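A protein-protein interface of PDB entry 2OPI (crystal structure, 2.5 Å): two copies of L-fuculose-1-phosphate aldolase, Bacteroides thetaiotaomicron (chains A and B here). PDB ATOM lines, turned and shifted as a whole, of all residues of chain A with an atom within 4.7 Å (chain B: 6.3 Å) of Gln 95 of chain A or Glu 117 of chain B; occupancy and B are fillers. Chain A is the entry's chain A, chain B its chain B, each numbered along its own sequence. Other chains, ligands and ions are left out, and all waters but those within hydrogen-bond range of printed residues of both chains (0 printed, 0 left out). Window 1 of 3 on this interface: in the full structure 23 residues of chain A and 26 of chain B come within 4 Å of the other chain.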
ATOM      1  N   LEU A  22     -19.046  -4.490  25.157  1.00  0.00           N
ATOM      2  CA  LEU A  22     -19.483  -5.724  24.497  1.00  0.00           C
ATOM      3  C   LEU A  22     -18.289  -6.609  24.121  1.00  0.00           C
ATOM      4  O   LEU A  22     -18.411  -7.828  24.031  1.00  0.00           O
ATOM      5  CB  LEU A  22     -20.335  -5.408  23.262  1.00  0.00           C
ATOM      6  CG  LEU A  22     -21.611  -4.562  23.421  1.00  0.00           C
ATOM      7  CD1 LEU A  22     -22.271  -4.409  22.069  1.00  0.00           C
ATOM      8  CD2 LEU A  22     -22.587  -5.153  24.400  1.00  0.00           C
ATOM      9  N   MET A  23     -17.143  -5.983  23.877  1.00  0.00           N
ATOM     10  CA  MET A  23     -15.867  -6.690  23.855  1.00  0.00           C
ATOM     11  C   MET A  23     -14.742  -5.871  24.477  1.00  0.00           C
ATOM     12  O   MET A  23     -14.882  -4.669  24.718  1.00  0.00           O
ATOM     13  CB  MET A  23     -15.451  -7.187  22.458  1.00  0.00           C
ATOM     14  CG  MET A  23     -16.243  -6.684  21.270  1.00  0.00           C
ATOM     15  SD  MET A  23     -16.332  -4.749  20.969  1.00  0.00           S
ATOM     16  CE  MET A  23     -17.149  -4.877  19.209  1.00  0.00           C
ATOM     17  N   SER A  27     -10.364  -8.859  21.110  1.00  0.00           N
ATOM     18  CA  SER A  27     -11.364  -9.907  20.892  1.00  0.00           C
ATOM     19  C   SER A  27     -12.608  -9.350  20.187  1.00  0.00           C
ATOM     20  O   SER A  27     -12.928  -8.165  20.314  1.00  0.00           O
ATOM     21  CB  SER A  27     -11.749 -10.593  22.200  1.00  0.00           C
ATOM     22  OG  SER A  27     -12.674  -9.797  22.917  1.00  0.00           O
ATOM     23  N   PHE A  94     -18.887 -10.695  19.616  1.00  0.00           N
ATOM     24  CA  PHE A  94     -18.427  -9.991  20.812  1.00  0.00           C
ATOM     25  C   PHE A  94     -18.193 -10.932  22.017  1.00  0.00           C
ATOM     26  O   PHE A  94     -18.174 -12.148  21.864  1.00  0.00           O
ATOM     27  CB  PHE A  94     -19.367  -8.814  21.132  1.00  0.00           C
ATOM     28  CG  PHE A  94     -20.762  -9.236  21.492  1.00  0.00           C
ATOM     29  CD1 PHE A  94     -21.590  -9.845  20.546  1.00  0.00           C
ATOM     30  CD2 PHE A  94     -21.237  -9.057  22.786  1.00  0.00           C
ATOM     31  CE1 PHE A  94     -22.874 -10.261  20.888  1.00  0.00           C
ATOM     32  CE2 PHE A  94     -22.518  -9.460  23.144  1.00  0.00           C
ATOM     33  CZ  PHE A  94     -23.341 -10.064  22.201  1.00  0.00           C
ATOM     34  N   GLN A  95     -17.989 -10.371  23.203  1.00  0.00           N
ATOM     35  CA  GLN A  95     -17.514 -11.139  24.347  1.00  0.00           C
ATOM     36  C   GLN A  95     -17.773 -10.355  25.634  1.00  0.00           C
ATOM     37  O   GLN A  95     -16.825  -9.901  26.289  1.00  0.00           O
ATOM     38  CB  GLN A  95     -16.010 -11.435  24.192  1.00  0.00           C
ATOM     39  CG  GLN A  95     -15.450 -12.492  25.152  1.00  0.00           C
ATOM     40  CD  GLN A  95     -13.966 -12.814  24.921  1.00  0.00           C
ATOM     41  OE1 GLN A  95     -13.102 -11.924  24.915  1.00  0.00           O
ATOM     42  NE2 GLN A  95     -13.669 -14.094  24.760  1.00  0.00           N
ATOM     43  N   SER A  96     -19.043 -10.176  25.990  1.00  0.00           N
ATOM     44  CA  SER A  96     -19.397  -9.336  27.131  1.00  0.00           C
ATOM     45  C   SER A  96     -19.338 -10.087  28.463  1.00  0.00           C
ATOM     46  O   SER A  96     -19.243 -11.311  28.490  1.00  0.00           O
ATOM     47  CB  SER A  96     -20.774  -8.723  26.929  1.00  0.00           C
ATOM     48  OG  SER A  96     -21.724  -9.733  26.656  1.00  0.00           O
ATOM     49  N   GLU A  97     -19.385  -9.332  29.558  1.00  0.00           N
ATOM     50  CA  GLU A  97     -19.318  -9.840  30.941  1.00  0.00           C
ATOM     51  C   GLU A  97     -20.111 -11.136  31.237  1.00  0.00           C
ATOM     52  O   GLU A  97     -19.544 -12.231  31.222  1.00  0.00           O
ATOM     53  CB  GLU A  97     -19.767  -8.722  31.883  1.00  0.00           C
ATOM     54  CG  GLU A  97     -19.386  -8.880  33.353  1.00  0.00           C
ATOM     55  CD  GLU A  97     -19.516  -7.562  34.115  1.00  0.00           C
ATOM     56  OE1 GLU A  97     -19.140  -7.493  35.305  1.00  0.00           O
ATOM     57  OE2 GLU A  97     -19.984  -6.579  33.515  1.00  0.00           O
ATOM     58  N   THR A 100     -20.370 -14.114  28.621  1.00  0.00           N
ATOM     59  CA  THR A 100     -19.186 -14.952  28.444  1.00  0.00           C
ATOM     60  C   THR A 100     -19.038 -15.941  29.608  1.00  0.00           C
ATOM     61  O   THR A 100     -18.615 -17.088  29.404  1.00  0.00           O
ATOM     62  CB  THR A 100     -17.915 -14.128  28.204  1.00  0.00           C
ATOM     63  OG1 THR A 100     -18.158 -13.199  27.141  1.00  0.00           O
ATOM     64  CG2 THR A 100     -16.767 -15.022  27.797  1.00  0.00           C
ATOM     65  N   HIS A 158     -16.129 -19.198  24.421  1.00  0.00           N
ATOM     66  CA  HIS A 158     -15.628 -18.096  23.652  1.00  0.00           C
ATOM     67  C   HIS A 158     -16.330 -16.762  23.770  1.00  0.00           C
ATOM     68  O   HIS A 158     -15.718 -15.802  24.234  1.00  0.00           O
ATOM     69  CB  HIS A 158     -15.390 -18.411  22.181  1.00  0.00           C
ATOM     70  CG  HIS A 158     -14.461 -17.423  21.575  1.00  0.00           C
ATOM     71  ND1 HIS A 158     -13.095 -17.464  21.807  1.00  0.00           N
ATOM     72  CD2 HIS A 158     -14.700 -16.269  20.913  1.00  0.00           C
ATOM     73  CE1 HIS A 158     -12.530 -16.414  21.239  1.00  0.00           C
ATOM     74  NE2 HIS A 158     -13.482 -15.674  20.690  1.00  0.00           N
ATOM     75  N   GLY A 159     -17.570 -16.679  23.303  1.00  0.00           N
ATOM     76  CA  GLY A 159     -18.305 -15.422  23.325  1.00  0.00           C
ATOM     77  C   GLY A 159     -19.670 -15.545  22.682  1.00  0.00           C
ATOM     78  O   GLY A 159     -20.391 -16.513  22.902  1.00  0.00           O
ATOM     79  N   GLN A 160     -20.031 -14.547  21.888  1.00  0.00           N
ATOM     80  CA  GLN A 160     -21.346 -14.541  21.270  1.00  0.00           C
ATOM     81  C   GLN A 160     -21.402 -13.813  19.930  1.00  0.00           C
ATOM     82  O   GLN A 160     -20.528 -13.011  19.599  1.00  0.00           O
ATOM     83  CB  GLN A 160     -22.451 -14.098  22.259  1.00  0.00           C
ATOM     84  CG  GLN A 160     -22.171 -12.912  23.182  1.00  0.00           C
ATOM     85  CD  GLN A 160     -21.203 -13.163  24.336  1.00  0.00           C
ATOM     86  OE1 GLN A 160     -20.335 -12.335  24.591  1.00  0.00           O
ATOM     87  NE2 GLN A 160     -21.348 -14.282  25.033  1.00  0.00           N
ATOM     88  N   THR B 115     -11.200 -19.047  27.715  1.00  0.00           N
ATOM     89  CA  THR B 115     -11.425 -18.641  26.329  1.00  0.00           C
ATOM     90  C   THR B 115     -10.084 -18.683  25.609  1.00  0.00           C
ATOM     91  O   THR B 115      -9.049 -18.860  26.249  1.00  0.00           O
ATOM     92  CB  THR B 115     -12.020 -17.210  26.189  1.00  0.00           C
ATOM     93  OG1 THR B 115     -11.005 -16.238  26.456  1.00  0.00           O
ATOM     94  CG2 THR B 115     -13.187 -16.979  27.123  1.00  0.00           C
ATOM     95  N   ALA B 116     -10.104 -18.506  24.290  1.00  0.00           N
ATOM     96  CA  ALA B 116      -8.883 -18.536  23.476  1.00  0.00           C
ATOM     97  C   ALA B 116      -7.870 -17.450  23.875  1.00  0.00           C
ATOM     98  O   ALA B 116      -6.664 -17.702  23.904  1.00  0.00           O
ATOM     99  CB  ALA B 116      -9.224 -18.421  21.995  1.00  0.00           C
ATOM    100  N   GLU B 117      -8.356 -16.250  24.182  1.00  0.00           N
ATOM    101  CA  GLU B 117      -7.452 -15.135  24.476  1.00  0.00           C
ATOM    102  C   GLU B 117      -6.593 -15.364  25.703  1.00  0.00           C
ATOM    103  O   GLU B 117      -5.539 -14.745  25.819  1.00  0.00           O
ATOM    104  CB  GLU B 117      -8.170 -13.775  24.568  1.00  0.00           C
ATOM    105  CG  GLU B 117      -9.644 -13.823  24.895  1.00  0.00           C
ATOM    106  CD  GLU B 117     -10.513 -14.274  23.709  1.00  0.00           C
ATOM    107  OE1 GLU B 117     -11.397 -15.140  23.917  1.00  0.00           O
ATOM    108  OE2 GLU B 117     -10.311 -13.775  22.574  1.00  0.00           O
ATOM    109  N   ILE B 118      -7.016 -16.265  26.593  1.00  0.00           N
ATOM    110  CA  ILE B 118      -6.280 -16.490  27.838  1.00  0.00           C
ATOM    111  C   ILE B 118      -4.942 -17.187  27.605  1.00  0.00           C
ATOM    112  O   ILE B 118      -3.907 -16.593  27.890  1.00  0.00           O
ATOM    113  CB  ILE B 118      -7.121 -17.173  28.952  1.00  0.00           C
ATOM    114  CG1 ILE B 118      -8.534 -16.572  29.012  1.00  0.00           C
ATOM    115  CG2 ILE B 118      -6.422 -17.046  30.300  1.00  0.00           C
ATOM    116  CD1 ILE B 118      -8.570 -15.100  29.428  1.00  0.00           C
ATOM    117  N   PRO B 119      -4.943 -18.419  27.058  1.00  0.00           N
ATOM    118  CA  PRO B 119      -3.649 -18.991  26.702  1.00  0.00           C
ATOM    119  C   PRO B 119      -2.824 -18.149  25.736  1.00  0.00           C
ATOM    120  O   PRO B 119      -1.602 -18.189  25.812  1.00  0.00           O
ATOM    121  CB  PRO B 119      -4.012 -20.340  26.066  1.00  0.00           C
ATOM    122  CG  PRO B 119      -5.450 -20.258  25.764  1.00  0.00           C
ATOM    123  CD  PRO B 119      -6.039 -19.362  26.781  1.00  0.00           C
ATOM    124  N   CYS B 120      -3.474 -17.386  24.855  1.00  0.00           N
ATOM    125  CA  CYS B 120      -2.748 -16.574  23.857  1.00  0.00           C
ATOM    126  C   CYS B 120      -2.065 -15.344  24.420  1.00  0.00           C
ATOM    127  O   CYS B 120      -0.930 -15.042  24.062  1.00  0.00           O
ATOM    128  CB  CYS B 120      -3.662 -16.128  22.727  1.00  0.00           C
ATOM    129  SG  CYS B 120      -3.999 -17.422  21.552  1.00  0.00           S
ATOM    130  N   HIS B 121      -2.761 -14.626  25.289  1.00  0.00           N
ATOM    131  CA  HIS B 121      -2.233 -13.369  25.788  1.00  0.00           C
ATOM    132  C   HIS B 121      -1.658 -13.502  27.187  1.00  0.00           C
ATOM    133  O   HIS B 121      -0.514 -13.128  27.416  1.00  0.00           O
ATOM    134  CB  HIS B 121      -3.291 -12.264  25.704  1.00  0.00           C
ATOM    135  CG  HIS B 121      -3.721 -11.962  24.303  1.00  0.00           C
ATOM    136  ND1 HIS B 121      -4.941 -12.352  23.797  1.00  0.00           N
ATOM    137  CD2 HIS B 121      -3.078 -11.336  23.288  1.00  0.00           C
ATOM    138  CE1 HIS B 121      -5.040 -11.969  22.535  1.00  0.00           C
ATOM    139  NE2 HIS B 121      -3.922 -11.350  22.203  1.00  0.00           N
ATOM    140  N   VAL B 122      -2.432 -14.073  28.103  1.00  0.00           N
ATOM    141  CA  VAL B 122      -2.035 -14.168  29.506  1.00  0.00           C
ATOM    142  C   VAL B 122      -0.988 -15.255  29.795  1.00  0.00           C
ATOM    143  O   VAL B 122      -0.160 -15.085  30.685  1.00  0.00           O
ATOM    144  CB  VAL B 122      -3.268 -14.365  30.419  1.00  0.00           C
ATOM    145  CG1 VAL B 122      -2.868 -14.372  31.884  1.00  0.00           C
ATOM    146  CG2 VAL B 122      -4.297 -13.271  30.170  1.00  0.00           C
ATOM    147  N   GLY B 123      -1.006 -16.345  29.030  1.00  0.00           N
ATOM    148  CA  GLY B 123      -0.170 -17.520  29.312  1.00  0.00           C
ATOM    149  C   GLY B 123      -1.036 -18.730  29.632  1.00  0.00           C
ATOM    150  O   GLY B 123      -2.100 -18.611  30.242  1.00  0.00           O
ATOM    151  N   PHE B 176      -7.239  -9.247  30.219  1.00  0.00           N
ATOM    152  CA  PHE B 176      -7.678 -10.625  29.998  1.00  0.00           C
ATOM    153  C   PHE B 176      -7.394 -11.498  31.221  1.00  0.00           C
ATOM    154  O   PHE B 176      -8.079 -12.484  31.472  1.00  0.00           O
ATOM    155  CB  PHE B 176      -7.042 -11.213  28.738  1.00  0.00           C
ATOM    156  CG  PHE B 176      -7.636 -10.705  27.447  1.00  0.00           C
ATOM    157  CD1 PHE B 176      -6.818 -10.443  26.351  1.00  0.00           C
ATOM    158  CD2 PHE B 176      -9.013 -10.518  27.308  1.00  0.00           C
ATOM    159  CE1 PHE B 176      -7.359  -9.994  25.128  1.00  0.00           C
ATOM    160  CE2 PHE B 176      -9.561 -10.053  26.105  1.00  0.00           C
ATOM    161  CZ  PHE B 176      -8.726  -9.789  25.010  1.00  0.00           C
ATOM    162  N   MET B 179     -10.330 -10.597  33.040  1.00  0.00           N
ATOM    163  CA  MET B 179     -11.514 -11.225  32.470  1.00  0.00           C
ATOM    164  C   MET B 179     -11.651 -12.720  32.816  1.00  0.00           C
ATOM    165  O   MET B 179     -12.735 -13.170  33.175  1.00  0.00           O
ATOM    166  CB  MET B 179     -11.576 -10.994  30.973  1.00  0.00           C
ATOM    167  CG  MET B 179     -12.741 -11.685  30.329  1.00  0.00           C
ATOM    168  SD  MET B 179     -12.638 -11.658  28.388  1.00  0.00           S
ATOM    169  CE  MET B 179     -14.233 -10.573  28.031  1.00  0.00           C
ATOM    170  N   LEU B 202      -4.316 -23.147  18.626  1.00  0.00           N
ATOM    171  CA  LEU B 202      -4.306 -21.690  18.553  1.00  0.00           C
ATOM    172  C   LEU B 202      -3.081 -21.074  17.853  1.00  0.00           C
ATOM    173  O   LEU B 202      -3.155 -19.941  17.383  1.00  0.00           O
ATOM    174  CB  LEU B 202      -4.511 -21.084  19.945  1.00  0.00           C
ATOM    175  CG  LEU B 202      -5.874 -21.295  20.618  1.00  0.00           C
ATOM    176  CD1 LEU B 202      -5.912 -20.669  22.002  1.00  0.00           C
ATOM    177  CD2 LEU B 202      -6.998 -20.738  19.783  1.00  0.00           C
ATOM    178  N   TYR B 205      -4.030 -19.911  14.548  1.00  0.00           N
ATOM    179  CA  TYR B 205      -4.806 -18.702  14.672  1.00  0.00           C
ATOM    180  C   TYR B 205      -3.891 -17.499  14.933  1.00  0.00           C
ATOM    181  O   TYR B 205      -4.047 -16.456  14.298  1.00  0.00           O
ATOM    182  CB  TYR B 205      -5.847 -18.874  15.774  1.00  0.00           C
ATOM    183  CG  TYR B 205      -6.668 -17.648  16.053  1.00  0.00           C
ATOM    184  CD1 TYR B 205      -7.483 -17.086  15.063  1.00  0.00           C
ATOM    185  CD2 TYR B 205      -6.654 -17.054  17.316  1.00  0.00           C
ATOM    186  CE1 TYR B 205      -8.255 -15.952  15.319  1.00  0.00           C
ATOM    187  CE2 TYR B 205      -7.422 -15.921  17.591  1.00  0.00           C
ATOM    188  CZ  TYR B 205      -8.219 -15.377  16.587  1.00  0.00           C
ATOM    189  OH  TYR B 205      -8.977 -14.261  16.854  1.00  0.00           O
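O of Leu 22 of chain A is in hydrogen-bond range of N of Gln 95 of chain A (2.7 Å).
The side-chain amide oxygen (OE1) of Gln 95 of chain A lies within hydrogen-bond range of the side-chain hydroxyl (OG) of Ser 27 of chain A, 2.9 Å away.
The backbone carbonyl oxygen of His 158 of chain A is in hydrogen-bond range of the side-chain amide nitrogen of Gln 95 of chain A (2.7 Å).
The side-chain hydroxyl (OG1) of Thr 115 of chain B sits at hydrogen-bond distance from the side-chain carboxylate (OE1) of Glu 117 of chain B (2.8 Å).
O of Ala 116 of chain B sits at hydrogen-bond distance from SG of Cys 120 of chain B, 3.6 Å away.
O of Glu 117 of chain B sits at hydrogen-bond distance from ND1 of His 121 of chain B, 3.2 Å away.
NE2 of Gln 95 of chain A is in hydrogen-bond range of OE1 of Glu 117 of chain B, 2.6 Å away.
The side-chain amide oxygen (OE1) of Gln 95 of chain A sits close to the side-chain sulfur (SD) of Met 179 of chain B (3.5 Å).
Of chain B, only Thr 115 (3.8 Å), Glu 117 (2.6 Å) and Met 179 (3.2 Å) come within 4 Å of Gln 95 of chain A.
Of chain A, only Ser 27, Gln 95 and His 158 come within 4 Å of Glu 117 of chain B.
Of the printed residues of chain A, Met 179 of chain B touches Gln 95 (3.2 Å).
Of the printed residues of chain B, His 158 of chain A touches Ala 116 and Glu 117.
Of the printed residues of chain A, Thr 115 of chain B touches Gln 95 (3.8 Å).
Met 23 of chain A touches none of the printed residues of chain B.
Val 122 of chain B touches none of the printed residues of chain A.
The nearest residue of chain B that does not touch Gln 95 of chain A is Phe 176 of chain B (4.2 Å).
The nearest printed residue of chain A that does not touch Glu 117 of chain B is Gly 159 of chain A (6.4 Å).
The nearest printed residue of chain A that does not touch Thr 115 of chain B is His 158 of chain A (4.02 Å).
Among the printed residues, merely in contact across the chains: His 158 of chain A with Glu 117 of chain B, Ser 27 of chain A with Glu 117 of chain B, Gln 95 of chain A with Thr 115 of chain B and His 158 of chain A with Ala 116 of chain B.
No position is printed for both chains.
Of the 13 printed residues of chain B, 4 touch a printed residue of chain A.
Printed residues of chain B that touch a printed residue of chain A: Thr 115, Ala 116, Glu 117 and Met 179.
Hydrophobic or aromatic side chains of chain B that line the printed part of chain A: Ala 116 and Met 179.
Printed residues of chain A that touch a printed residue of chain B: Ser 27, Gln 95 and His 158.
Among the printed residues, 6 pairs touch across the chains.
Among the printed residues, no Asp or Glu carboxylate lies within 4 Å of a Lys or Arg side-chain nitrogen of the other chain.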
